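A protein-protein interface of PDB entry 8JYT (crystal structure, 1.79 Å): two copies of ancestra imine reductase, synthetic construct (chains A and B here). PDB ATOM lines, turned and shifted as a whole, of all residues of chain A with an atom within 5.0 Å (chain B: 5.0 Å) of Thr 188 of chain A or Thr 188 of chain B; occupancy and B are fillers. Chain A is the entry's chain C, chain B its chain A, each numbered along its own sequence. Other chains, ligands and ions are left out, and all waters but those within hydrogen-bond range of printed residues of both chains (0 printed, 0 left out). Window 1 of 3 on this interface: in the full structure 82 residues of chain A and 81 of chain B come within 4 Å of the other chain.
O of Asp 183 of chain B is in hydrogen-bond range of OG1 of Thr 187 of chain B (2.9 Å).
The backbone carbonyl oxygen (O) of Ile 184 of chain B lies within hydrogen-bond range of the side-chain hydroxyl (OG1) of Thr 188 of chain B (2.8 Å).
The side-chain hydroxyl (OG1) of Thr 188 of chain A lies within hydrogen-bond range of the backbone carbonyl oxygen (O) of Ile 184 of chain A (2.8 Å).
The backbone carbonyl oxygen of Asp 183 of chain A sits at hydrogen-bond distance from the side-chain hydroxyl of Thr 187 of chain A.
CG2 of Thr 187 of chain A touches CB of Ala 191 of chain B (3.5 Å).
OG1 of Thr 188 of chain A touches CG2 of Thr 188 of chain B, at 3.7 Å.
Thr 188 of chain A touches Phe 217 of chain B (OG1 to CE1, 3.7 Å).
CG2 of Thr 188 of chain A touches CE of Met 220 of chain B, 3.7 Å away.
CG of Met 220 of chain B touches CE of Met 189 of chain A, at 3.6 Å.
Ile 184 of chain B touches Ala 191 of chain A.
Ala 191 of chain A touches Thr 187 of chain B.
Phe 217 of chain A touches Ile 184 of chain B.
Phe 185 of chain B touches Met 220 of chain A (CA to CE, 3.97 Å).
SD of Met 220 of chain A touches CE of Met 189 of chain B, 3.4 Å away.
Thr 188 of chain A touches just these residues of chain B: Thr 188, Phe 217 and Met 220.
Of chain A, only Thr 188 (3.7 Å), Phe 217 (3.4 Å) and Met 220 (3.9 Å) come within 4 Å of Thr 188 of chain B.
Of the printed residues of chain B, Met 220 of chain A touches Phe 185 (3.97 Å), Thr 188 (3.9 Å) and Met 189 (3.4 Å).
Printed residues of chain B within 4 Å of Thr 187 of chain A: Ala 191.
Printed residues of chain B within 4 Å of Phe 217 of chain A: Ile 184 (3.4 Å) and Thr 188 (3.4 Å).
Of the printed residues of chain A, Met 220 of chain B touches Thr 188 (3.7 Å) and Met 189 (3.6 Å).
Phe 185 of chain A touches none of the printed residues of chain B.
The nearest residue of chain A that does not touch Thr 188 of chain B is Ala 191 of chain A (4.3 Å).
Hydrophobic or aromatic side chains of chain B that line the printed part of chain A: Ile 184, Met 189, Ala 191, Phe 217 and Met 220.
Printed residues of chain A that touch a printed residue of chain B: Ile 184, Thr 187, Thr 188, Met 189, Ala 191, Phe 217 and Met 220.
Among the printed residues, no Asp or Glu carboxylate lies within 4 Å of a Lys or Arg side-chain nitrogen of the other chain.
Ile 184 of chain A touches Phe 217 of chain B, and with the chains exchanged Phe 217 of chain A touches Ile 184 of chain B.
Thr 187 of chain A touches Ala 191 of chain B, and with the chains exchanged Ala 191 of chain A touches Thr 187 of chain B.
Thr 188 of chain A touches Met 220 of chain B, and with the chains exchanged Met 220 of chain A touches Thr 188 of chain B.
Met 189 of chain A touches Met 220 of chain B, and with the chains exchanged Met 220 of chain A touches Met 189 of chain B.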
ATOM      1  N   ASP A 183       1.180  22.713  24.483  1.00  0.00           N
ATOM      2  CA  ASP A 183      -0.273  22.819  24.460  1.00  0.00           C
ATOM      3  C   ASP A 183      -0.711  23.992  23.583  1.00  0.00           C
ATOM      4  O   ASP A 183      -1.663  23.881  22.793  1.00  0.00           O
ATOM      5  CB  ASP A 183      -0.728  22.971  25.912  1.00  0.00           C
ATOM      6  CG  ASP A 183      -2.221  23.056  26.073  1.00  0.00           C
ATOM      7  OD1 ASP A 183      -2.952  22.576  25.179  1.00  0.00           O
ATOM      8  OD2 ASP A 183      -2.648  23.499  27.163  1.00  0.00           O
ATOM      9  N   ILE A 184       0.004  25.115  23.690  1.00  0.00           N
ATOM     10  CA  ILE A 184      -0.240  26.246  22.805  1.00  0.00           C
ATOM     11  C   ILE A 184       0.117  25.862  21.376  1.00  0.00           C
ATOM     12  O   ILE A 184      -0.657  26.075  20.438  1.00  0.00           O
ATOM     13  CB  ILE A 184       0.574  27.464  23.270  1.00  0.00           C
ATOM     14  CG1 ILE A 184      -0.050  28.049  24.533  1.00  0.00           C
ATOM     15  CG2 ILE A 184       0.643  28.478  22.134  1.00  0.00           C
ATOM     16  CD1 ILE A 184       0.717  29.208  25.109  1.00  0.00           C
ATOM     17  N   PHE A 185       1.291  25.257  21.200  1.00  0.00           N
ATOM     18  CA  PHE A 185       1.780  24.920  19.865  1.00  0.00           C
ATOM     19  C   PHE A 185       0.813  24.004  19.115  1.00  0.00           C
ATOM     20  O   PHE A 185       0.340  24.340  18.028  1.00  0.00           O
ATOM     21  CB  PHE A 185       3.151  24.259  19.970  1.00  0.00           C
ATOM     22  CG  PHE A 185       3.751  23.927  18.645  1.00  0.00           C
ATOM     23  CD1 PHE A 185       4.264  24.922  17.842  1.00  0.00           C
ATOM     24  CD2 PHE A 185       3.819  22.614  18.206  1.00  0.00           C
ATOM     25  CE1 PHE A 185       4.824  24.615  16.626  1.00  0.00           C
ATOM     26  CE2 PHE A 185       4.363  22.314  16.990  1.00  0.00           C
ATOM     27  CZ  PHE A 185       4.863  23.311  16.196  1.00  0.00           C
ATOM     28  N   TRP A 186       0.557  22.805  19.652  1.00  0.00           N
ATOM     29  CA  TRP A 186      -0.219  21.827  18.898  1.00  0.00           C
ATOM     30  C   TRP A 186      -1.649  22.301  18.674  1.00  0.00           C
ATOM     31  O   TRP A 186      -2.206  22.099  17.594  1.00  0.00           O
ATOM     32  CB  TRP A 186      -0.218  20.471  19.609  1.00  0.00           C
ATOM     33  CG  TRP A 186       1.091  19.756  19.488  1.00  0.00           C
ATOM     34  CD1 TRP A 186       1.863  19.285  20.512  1.00  0.00           C
ATOM     35  CD2 TRP A 186       1.775  19.404  18.278  1.00  0.00           C
ATOM     36  NE1 TRP A 186       2.989  18.685  20.016  1.00  0.00           N
ATOM     37  CE2 TRP A 186       2.957  18.734  18.649  1.00  0.00           C
ATOM     38  CE3 TRP A 186       1.501  19.581  16.921  1.00  0.00           C
ATOM     39  CZ2 TRP A 186       3.872  18.258  17.716  1.00  0.00           C
ATOM     40  CZ3 TRP A 186       2.412  19.103  15.993  1.00  0.00           C
ATOM     41  CH2 TRP A 186       3.581  18.443  16.398  1.00  0.00           C
ATOM     42  N   THR A 187      -2.276  22.897  19.693  1.00  0.00           N
ATOM     43  CA  THR A 187      -3.646  23.374  19.505  1.00  0.00           C
ATOM     44  C   THR A 187      -3.707  24.489  18.473  1.00  0.00           C
ATOM     45  O   THR A 187      -4.638  24.525  17.655  1.00  0.00           O
ATOM     46  CB  THR A 187      -4.243  23.838  20.831  1.00  0.00           C
ATOM     47  OG1 THR A 187      -4.088  22.785  21.783  1.00  0.00           O
ATOM     48  CG2 THR A 187      -5.716  24.141  20.699  1.00  0.00           C
ATOM     49  N   THR A 188      -2.714  25.387  18.479  1.00  0.00           N
ATOM     50  CA  THR A 188      -2.673  26.472  17.499  1.00  0.00           C
ATOM     51  C   THR A 188      -2.382  25.936  16.105  1.00  0.00           C
ATOM     52  O   THR A 188      -2.973  26.396  15.124  1.00  0.00           O
ATOM     53  CB  THR A 188      -1.620  27.507  17.894  1.00  0.00           C
ATOM     54  OG1 THR A 188      -1.991  28.122  19.132  1.00  0.00           O
ATOM     55  CG2 THR A 188      -1.492  28.590  16.832  1.00  0.00           C
ATOM     56  N   MET A 189      -1.494  24.943  15.991  1.00  0.00           N
ATOM     57  CA  MET A 189      -1.255  24.340  14.683  1.00  0.00           C
ATOM     58  C   MET A 189      -2.520  23.697  14.132  1.00  0.00           C
ATOM     59  O   MET A 189      -2.816  23.819  12.941  1.00  0.00           O
ATOM     60  CB  MET A 189      -0.144  23.292  14.763  1.00  0.00           C
ATOM     61  CG  MET A 189       1.243  23.854  15.003  1.00  0.00           C
ATOM     62  SD  MET A 189       1.879  24.785  13.605  1.00  0.00           S
ATOM     63  CE  MET A 189       1.433  26.428  14.099  1.00  0.00           C
ATOM     64  N   THR A 190      -3.252  22.965  14.974  1.00  0.00           N
ATOM     65  CA  THR A 190      -4.505  22.359  14.537  1.00  0.00           C
ATOM     66  C   THR A 190      -5.519  23.417  14.104  1.00  0.00           C
ATOM     67  O   THR A 190      -6.255  23.221  13.125  1.00  0.00           O
ATOM     68  CB  THR A 190      -5.057  21.484  15.666  1.00  0.00           C
ATOM     69  OG1 THR A 190      -4.054  20.540  16.077  1.00  0.00           O
ATOM     70  CG2 THR A 190      -6.288  20.729  15.226  1.00  0.00           C
ATOM     71  N   ALA A 191      -5.560  24.554  14.804  1.00  0.00           N
ATOM     72  CA  ALA A 191      -6.474  25.622  14.406  1.00  0.00           C
ATOM     73  C   ALA A 191      -6.107  26.166  13.029  1.00  0.00           C
ATOM     74  O   ALA A 191      -6.984  26.377  12.184  1.00  0.00           O
ATOM     75  CB  ALA A 191      -6.484  26.745  15.447  1.00  0.00           C
ATOM     76  N   TYR A 192      -4.818  26.407  12.786  1.00  0.00           N
ATOM     77  CA  TYR A 192      -4.381  26.874  11.473  1.00  0.00           C
ATOM     78  C   TYR A 192      -4.767  25.885  10.377  1.00  0.00           C
ATOM     79  O   TYR A 192      -5.243  26.279   9.312  1.00  0.00           O
ATOM     80  CB  TYR A 192      -2.865  27.090  11.477  1.00  0.00           C
ATOM     81  CG  TYR A 192      -2.278  27.231  10.091  1.00  0.00           C
ATOM     82  CD1 TYR A 192      -2.492  28.385   9.345  1.00  0.00           C
ATOM     83  CD2 TYR A 192      -1.544  26.199   9.506  1.00  0.00           C
ATOM     84  CE1 TYR A 192      -1.984  28.511   8.062  1.00  0.00           C
ATOM     85  CE2 TYR A 192      -1.040  26.323   8.218  1.00  0.00           C
ATOM     86  CZ  TYR A 192      -1.267  27.489   7.509  1.00  0.00           C
ATOM     87  OH  TYR A 192      -0.766  27.633   6.242  1.00  0.00           O
ATOM     88  N   PHE A 217      -2.274  36.173  13.682  1.00  0.00           N
ATOM     89  CA  PHE A 217      -1.413  35.933  14.834  1.00  0.00           C
ATOM     90  C   PHE A 217      -0.654  37.193  15.235  1.00  0.00           C
ATOM     91  O   PHE A 217      -0.430  37.425  16.428  1.00  0.00           O
ATOM     92  CB  PHE A 217      -0.446  34.799  14.506  1.00  0.00           C
ATOM     93  CG  PHE A 217      -1.104  33.445  14.464  1.00  0.00           C
ATOM     94  CD1 PHE A 217      -1.785  32.953  15.562  1.00  0.00           C
ATOM     95  CD2 PHE A 217      -1.036  32.665  13.324  1.00  0.00           C
ATOM     96  CE1 PHE A 217      -2.388  31.713  15.524  1.00  0.00           C
ATOM     97  CE2 PHE A 217      -1.638  31.417  13.277  1.00  0.00           C
ATOM     98  CZ  PHE A 217      -2.314  30.940  14.381  1.00  0.00           C
ATOM     99  N   MET A 220      -2.555  39.536  17.689  1.00  0.00           N
ATOM    100  CA  MET A 220      -2.737  39.129  19.083  1.00  0.00           C
ATOM    101  C   MET A 220      -1.654  39.805  19.920  1.00  0.00           C
ATOM    102  O   MET A 220      -0.668  39.193  20.352  1.00  0.00           O
ATOM    103  CB  MET A 220      -2.693  37.611  19.193  1.00  0.00           C
ATOM    104  CG  MET A 220      -3.581  36.902  18.171  1.00  0.00           C
ATOM    105  SD  MET A 220      -3.531  35.097  18.303  1.00  0.00           S
ATOM    106  CE  MET A 220      -4.922  34.656  17.247  1.00  0.00           C
ATOM    107  N   ASP B 183     -11.939  31.331  13.370  1.00  0.00           N
ATOM    108  CA  ASP B 183     -11.603  29.965  13.756  1.00  0.00           C
ATOM    109  C   ASP B 183     -10.204  29.899  14.367  1.00  0.00           C
ATOM    110  O   ASP B 183     -10.006  29.344  15.460  1.00  0.00           O
ATOM    111  CB  ASP B 183     -11.766  29.123  12.495  1.00  0.00           C
ATOM    112  CG  ASP B 183     -11.567  27.634  12.710  1.00  0.00           C
ATOM    113  OD1 ASP B 183     -11.735  27.142  13.848  1.00  0.00           O
ATOM    114  OD2 ASP B 183     -11.365  26.958  11.681  1.00  0.00           O
ATOM    115  N   ILE B 184      -9.245  30.563  13.727  1.00  0.00           N
ATOM    116  CA  ILE B 184      -7.914  30.667  14.296  1.00  0.00           C
ATOM    117  C   ILE B 184      -7.949  31.458  15.592  1.00  0.00           C
ATOM    118  O   ILE B 184      -7.330  31.071  16.585  1.00  0.00           O
ATOM    119  CB  ILE B 184      -6.947  31.294  13.282  1.00  0.00           C
ATOM    120  CG1 ILE B 184      -6.705  30.340  12.112  1.00  0.00           C
ATOM    121  CG2 ILE B 184      -5.639  31.641  13.956  1.00  0.00           C
ATOM    122  CD1 ILE B 184      -6.026  30.983  10.945  1.00  0.00           C
ATOM    123  N   PHE B 185      -8.689  32.568  15.611  1.00  0.00           N
ATOM    124  CA  PHE B 185      -8.668  33.446  16.770  1.00  0.00           C
ATOM    125  C   PHE B 185      -9.164  32.737  18.016  1.00  0.00           C
ATOM    126  O   PHE B 185      -8.460  32.660  19.025  1.00  0.00           O
ATOM    127  CB  PHE B 185      -9.532  34.663  16.517  1.00  0.00           C
ATOM    128  CG  PHE B 185      -9.689  35.535  17.724  1.00  0.00           C
ATOM    129  CD1 PHE B 185      -8.622  36.268  18.213  1.00  0.00           C
ATOM    130  CD2 PHE B 185     -10.885  35.570  18.413  1.00  0.00           C
ATOM    131  CE1 PHE B 185      -8.774  37.064  19.318  1.00  0.00           C
ATOM    132  CE2 PHE B 185     -11.027  36.357  19.550  1.00  0.00           C
ATOM    133  CZ  PHE B 185      -9.991  37.103  19.985  1.00  0.00           C
ATOM    134  N   TRP B 186     -10.395  32.238  17.978  1.00  0.00           N
ATOM    135  CA  TRP B 186     -10.984  31.694  19.189  1.00  0.00           C
ATOM    136  C   TRP B 186     -10.289  30.415  19.634  1.00  0.00           C
ATOM    137  O   TRP B 186     -10.115  30.200  20.834  1.00  0.00           O
ATOM    138  CB  TRP B 186     -12.470  31.458  18.979  1.00  0.00           C
ATOM    139  CG  TRP B 186     -13.234  32.730  18.908  1.00  0.00           C
ATOM    140  CD1 TRP B 186     -13.906  33.229  17.840  1.00  0.00           C
ATOM    141  CD2 TRP B 186     -13.384  33.684  19.968  1.00  0.00           C
ATOM    142  NE1 TRP B 186     -14.478  34.442  18.164  1.00  0.00           N
ATOM    143  CE2 TRP B 186     -14.166  34.745  19.465  1.00  0.00           C
ATOM    144  CE3 TRP B 186     -12.918  33.750  21.291  1.00  0.00           C
ATOM    145  CZ2 TRP B 186     -14.504  35.856  20.236  1.00  0.00           C
ATOM    146  CZ3 TRP B 186     -13.262  34.849  22.064  1.00  0.00           C
ATOM    147  CH2 TRP B 186     -14.049  35.893  21.529  1.00  0.00           C
ATOM    148  N   THR B 187      -9.908  29.548  18.693  1.00  0.00           N
ATOM    149  CA  THR B 187      -9.215  28.318  19.074  1.00  0.00           C
ATOM    150  C   THR B 187      -7.840  28.618  19.679  1.00  0.00           C
ATOM    151  O   THR B 187      -7.444  28.017  20.689  1.00  0.00           O
ATOM    152  CB  THR B 187      -9.088  27.405  17.854  1.00  0.00           C
ATOM    153  OG1 THR B 187     -10.380  27.179  17.280  1.00  0.00           O
ATOM    154  CG2 THR B 187      -8.498  26.077  18.279  1.00  0.00           C
ATOM    155  N   THR B 188      -7.095  29.552  19.077  1.00  0.00           N
ATOM    156  CA  THR B 188      -5.799  29.944  19.626  1.00  0.00           C
ATOM    157  C   THR B 188      -5.954  30.627  20.980  1.00  0.00           C
ATOM    158  O   THR B 188      -5.136  30.424  21.886  1.00  0.00           O
ATOM    159  CB  THR B 188      -5.071  30.876  18.657  1.00  0.00           C
ATOM    160  OG1 THR B 188      -4.811  30.199  17.425  1.00  0.00           O
ATOM    161  CG2 THR B 188      -3.739  31.333  19.258  1.00  0.00           C
ATOM    162  N   MET B 189      -6.988  31.454  21.135  1.00  0.00           N
ATOM    163  CA  MET B 189      -7.236  32.073  22.434  1.00  0.00           C
ATOM    164  C   MET B 189      -7.555  31.017  23.492  1.00  0.00           C
ATOM    165  O   MET B 189      -7.082  31.104  24.633  1.00  0.00           O
ATOM    166  CB  MET B 189      -8.385  33.071  22.327  1.00  0.00           C
ATOM    167  CG  MET B 189      -8.060  34.341  21.556  1.00  0.00           C
ATOM    168  SD  MET B 189      -6.752  35.342  22.296  1.00  0.00           S
ATOM    169  CE  MET B 189      -5.378  34.960  21.207  1.00  0.00           C
ATOM    170  N   THR B 190      -8.389  30.034  23.141  1.00  0.00           N
ATOM    171  CA  THR B 190      -8.708  28.952  24.070  1.00  0.00           C
ATOM    172  C   THR B 190      -7.455  28.184  24.459  1.00  0.00           C
ATOM    173  O   THR B 190      -7.293  27.780  25.619  1.00  0.00           O
ATOM    174  CB  THR B 190      -9.742  28.026  23.423  1.00  0.00           C
ATOM    175  OG1 THR B 190     -10.928  28.780  23.143  1.00  0.00           O
ATOM    176  CG2 THR B 190     -10.113  26.889  24.334  1.00  0.00           C
ATOM    177  N   ALA B 191      -6.552  27.970  23.499  1.00  0.00           N
ATOM    178  CA  ALA B 191      -5.308  27.272  23.792  1.00  0.00           C
ATOM    179  C   ALA B 191      -4.430  28.085  24.732  1.00  0.00           C
ATOM    180  O   ALA B 191      -3.851  27.543  25.677  1.00  0.00           O
ATOM    181  CB  ALA B 191      -4.558  26.968  22.500  1.00  0.00           C
ATOM    182  N   TYR B 192      -4.289  29.384  24.465  1.00  0.00           N
ATOM    183  CA  TYR B 192      -3.501  30.233  25.345  1.00  0.00           C
ATOM    184  C   TYR B 192      -4.026  30.187  26.773  1.00  0.00           C
ATOM    185  O   TYR B 192      -3.245  30.098  27.721  1.00  0.00           O
ATOM    186  CB  TYR B 192      -3.504  31.669  24.822  1.00  0.00           C
ATOM    187  CG  TYR B 192      -3.005  32.654  25.853  1.00  0.00           C
ATOM    188  CD1 TYR B 192      -1.644  32.841  26.048  1.00  0.00           C
ATOM    189  CD2 TYR B 192      -3.890  33.387  26.649  1.00  0.00           C
ATOM    190  CE1 TYR B 192      -1.176  33.717  26.987  1.00  0.00           C
ATOM    191  CE2 TYR B 192      -3.414  34.283  27.602  1.00  0.00           C
ATOM    192  CZ  TYR B 192      -2.058  34.434  27.762  1.00  0.00           C
ATOM    193  OH  TYR B 192      -1.557  35.296  28.711  1.00  0.00           O
ATOM    194  N   PHE B 217       4.536  31.885  19.917  1.00  0.00           N
ATOM    195  CA  PHE B 217       3.837  32.413  18.754  1.00  0.00           C
ATOM    196  C   PHE B 217       4.806  33.075  17.784  1.00  0.00           C
ATOM    197  O   PHE B 217       4.668  32.935  16.564  1.00  0.00           O
ATOM    198  CB  PHE B 217       2.776  33.400  19.221  1.00  0.00           C
ATOM    199  CG  PHE B 217       1.654  32.773  20.003  1.00  0.00           C
ATOM    200  CD1 PHE B 217       0.914  31.729  19.473  1.00  0.00           C
ATOM    201  CD2 PHE B 217       1.339  33.231  21.275  1.00  0.00           C
ATOM    202  CE1 PHE B 217      -0.128  31.168  20.187  1.00  0.00           C
ATOM    203  CE2 PHE B 217       0.306  32.662  22.000  1.00  0.00           C
ATOM    204  CZ  PHE B 217      -0.429  31.635  21.454  1.00  0.00           C
ATOM    205  N   MET B 220       6.512  30.609  15.404  1.00  0.00           N
ATOM    206  CA  MET B 220       5.741  30.000  14.310  1.00  0.00           C
ATOM    207  C   MET B 220       6.068  30.725  13.000  1.00  0.00           C
ATOM    208  O   MET B 220       5.368  31.630  12.546  1.00  0.00           O
ATOM    209  CB  MET B 220       4.245  30.014  14.637  1.00  0.00           C
ATOM    210  CG  MET B 220       3.803  28.771  15.435  1.00  0.00           C
ATOM    211  SD  MET B 220       2.517  29.061  16.661  1.00  0.00           S
ATOM    212  CE  MET B 220       1.606  30.422  15.925  1.00  0.00           C
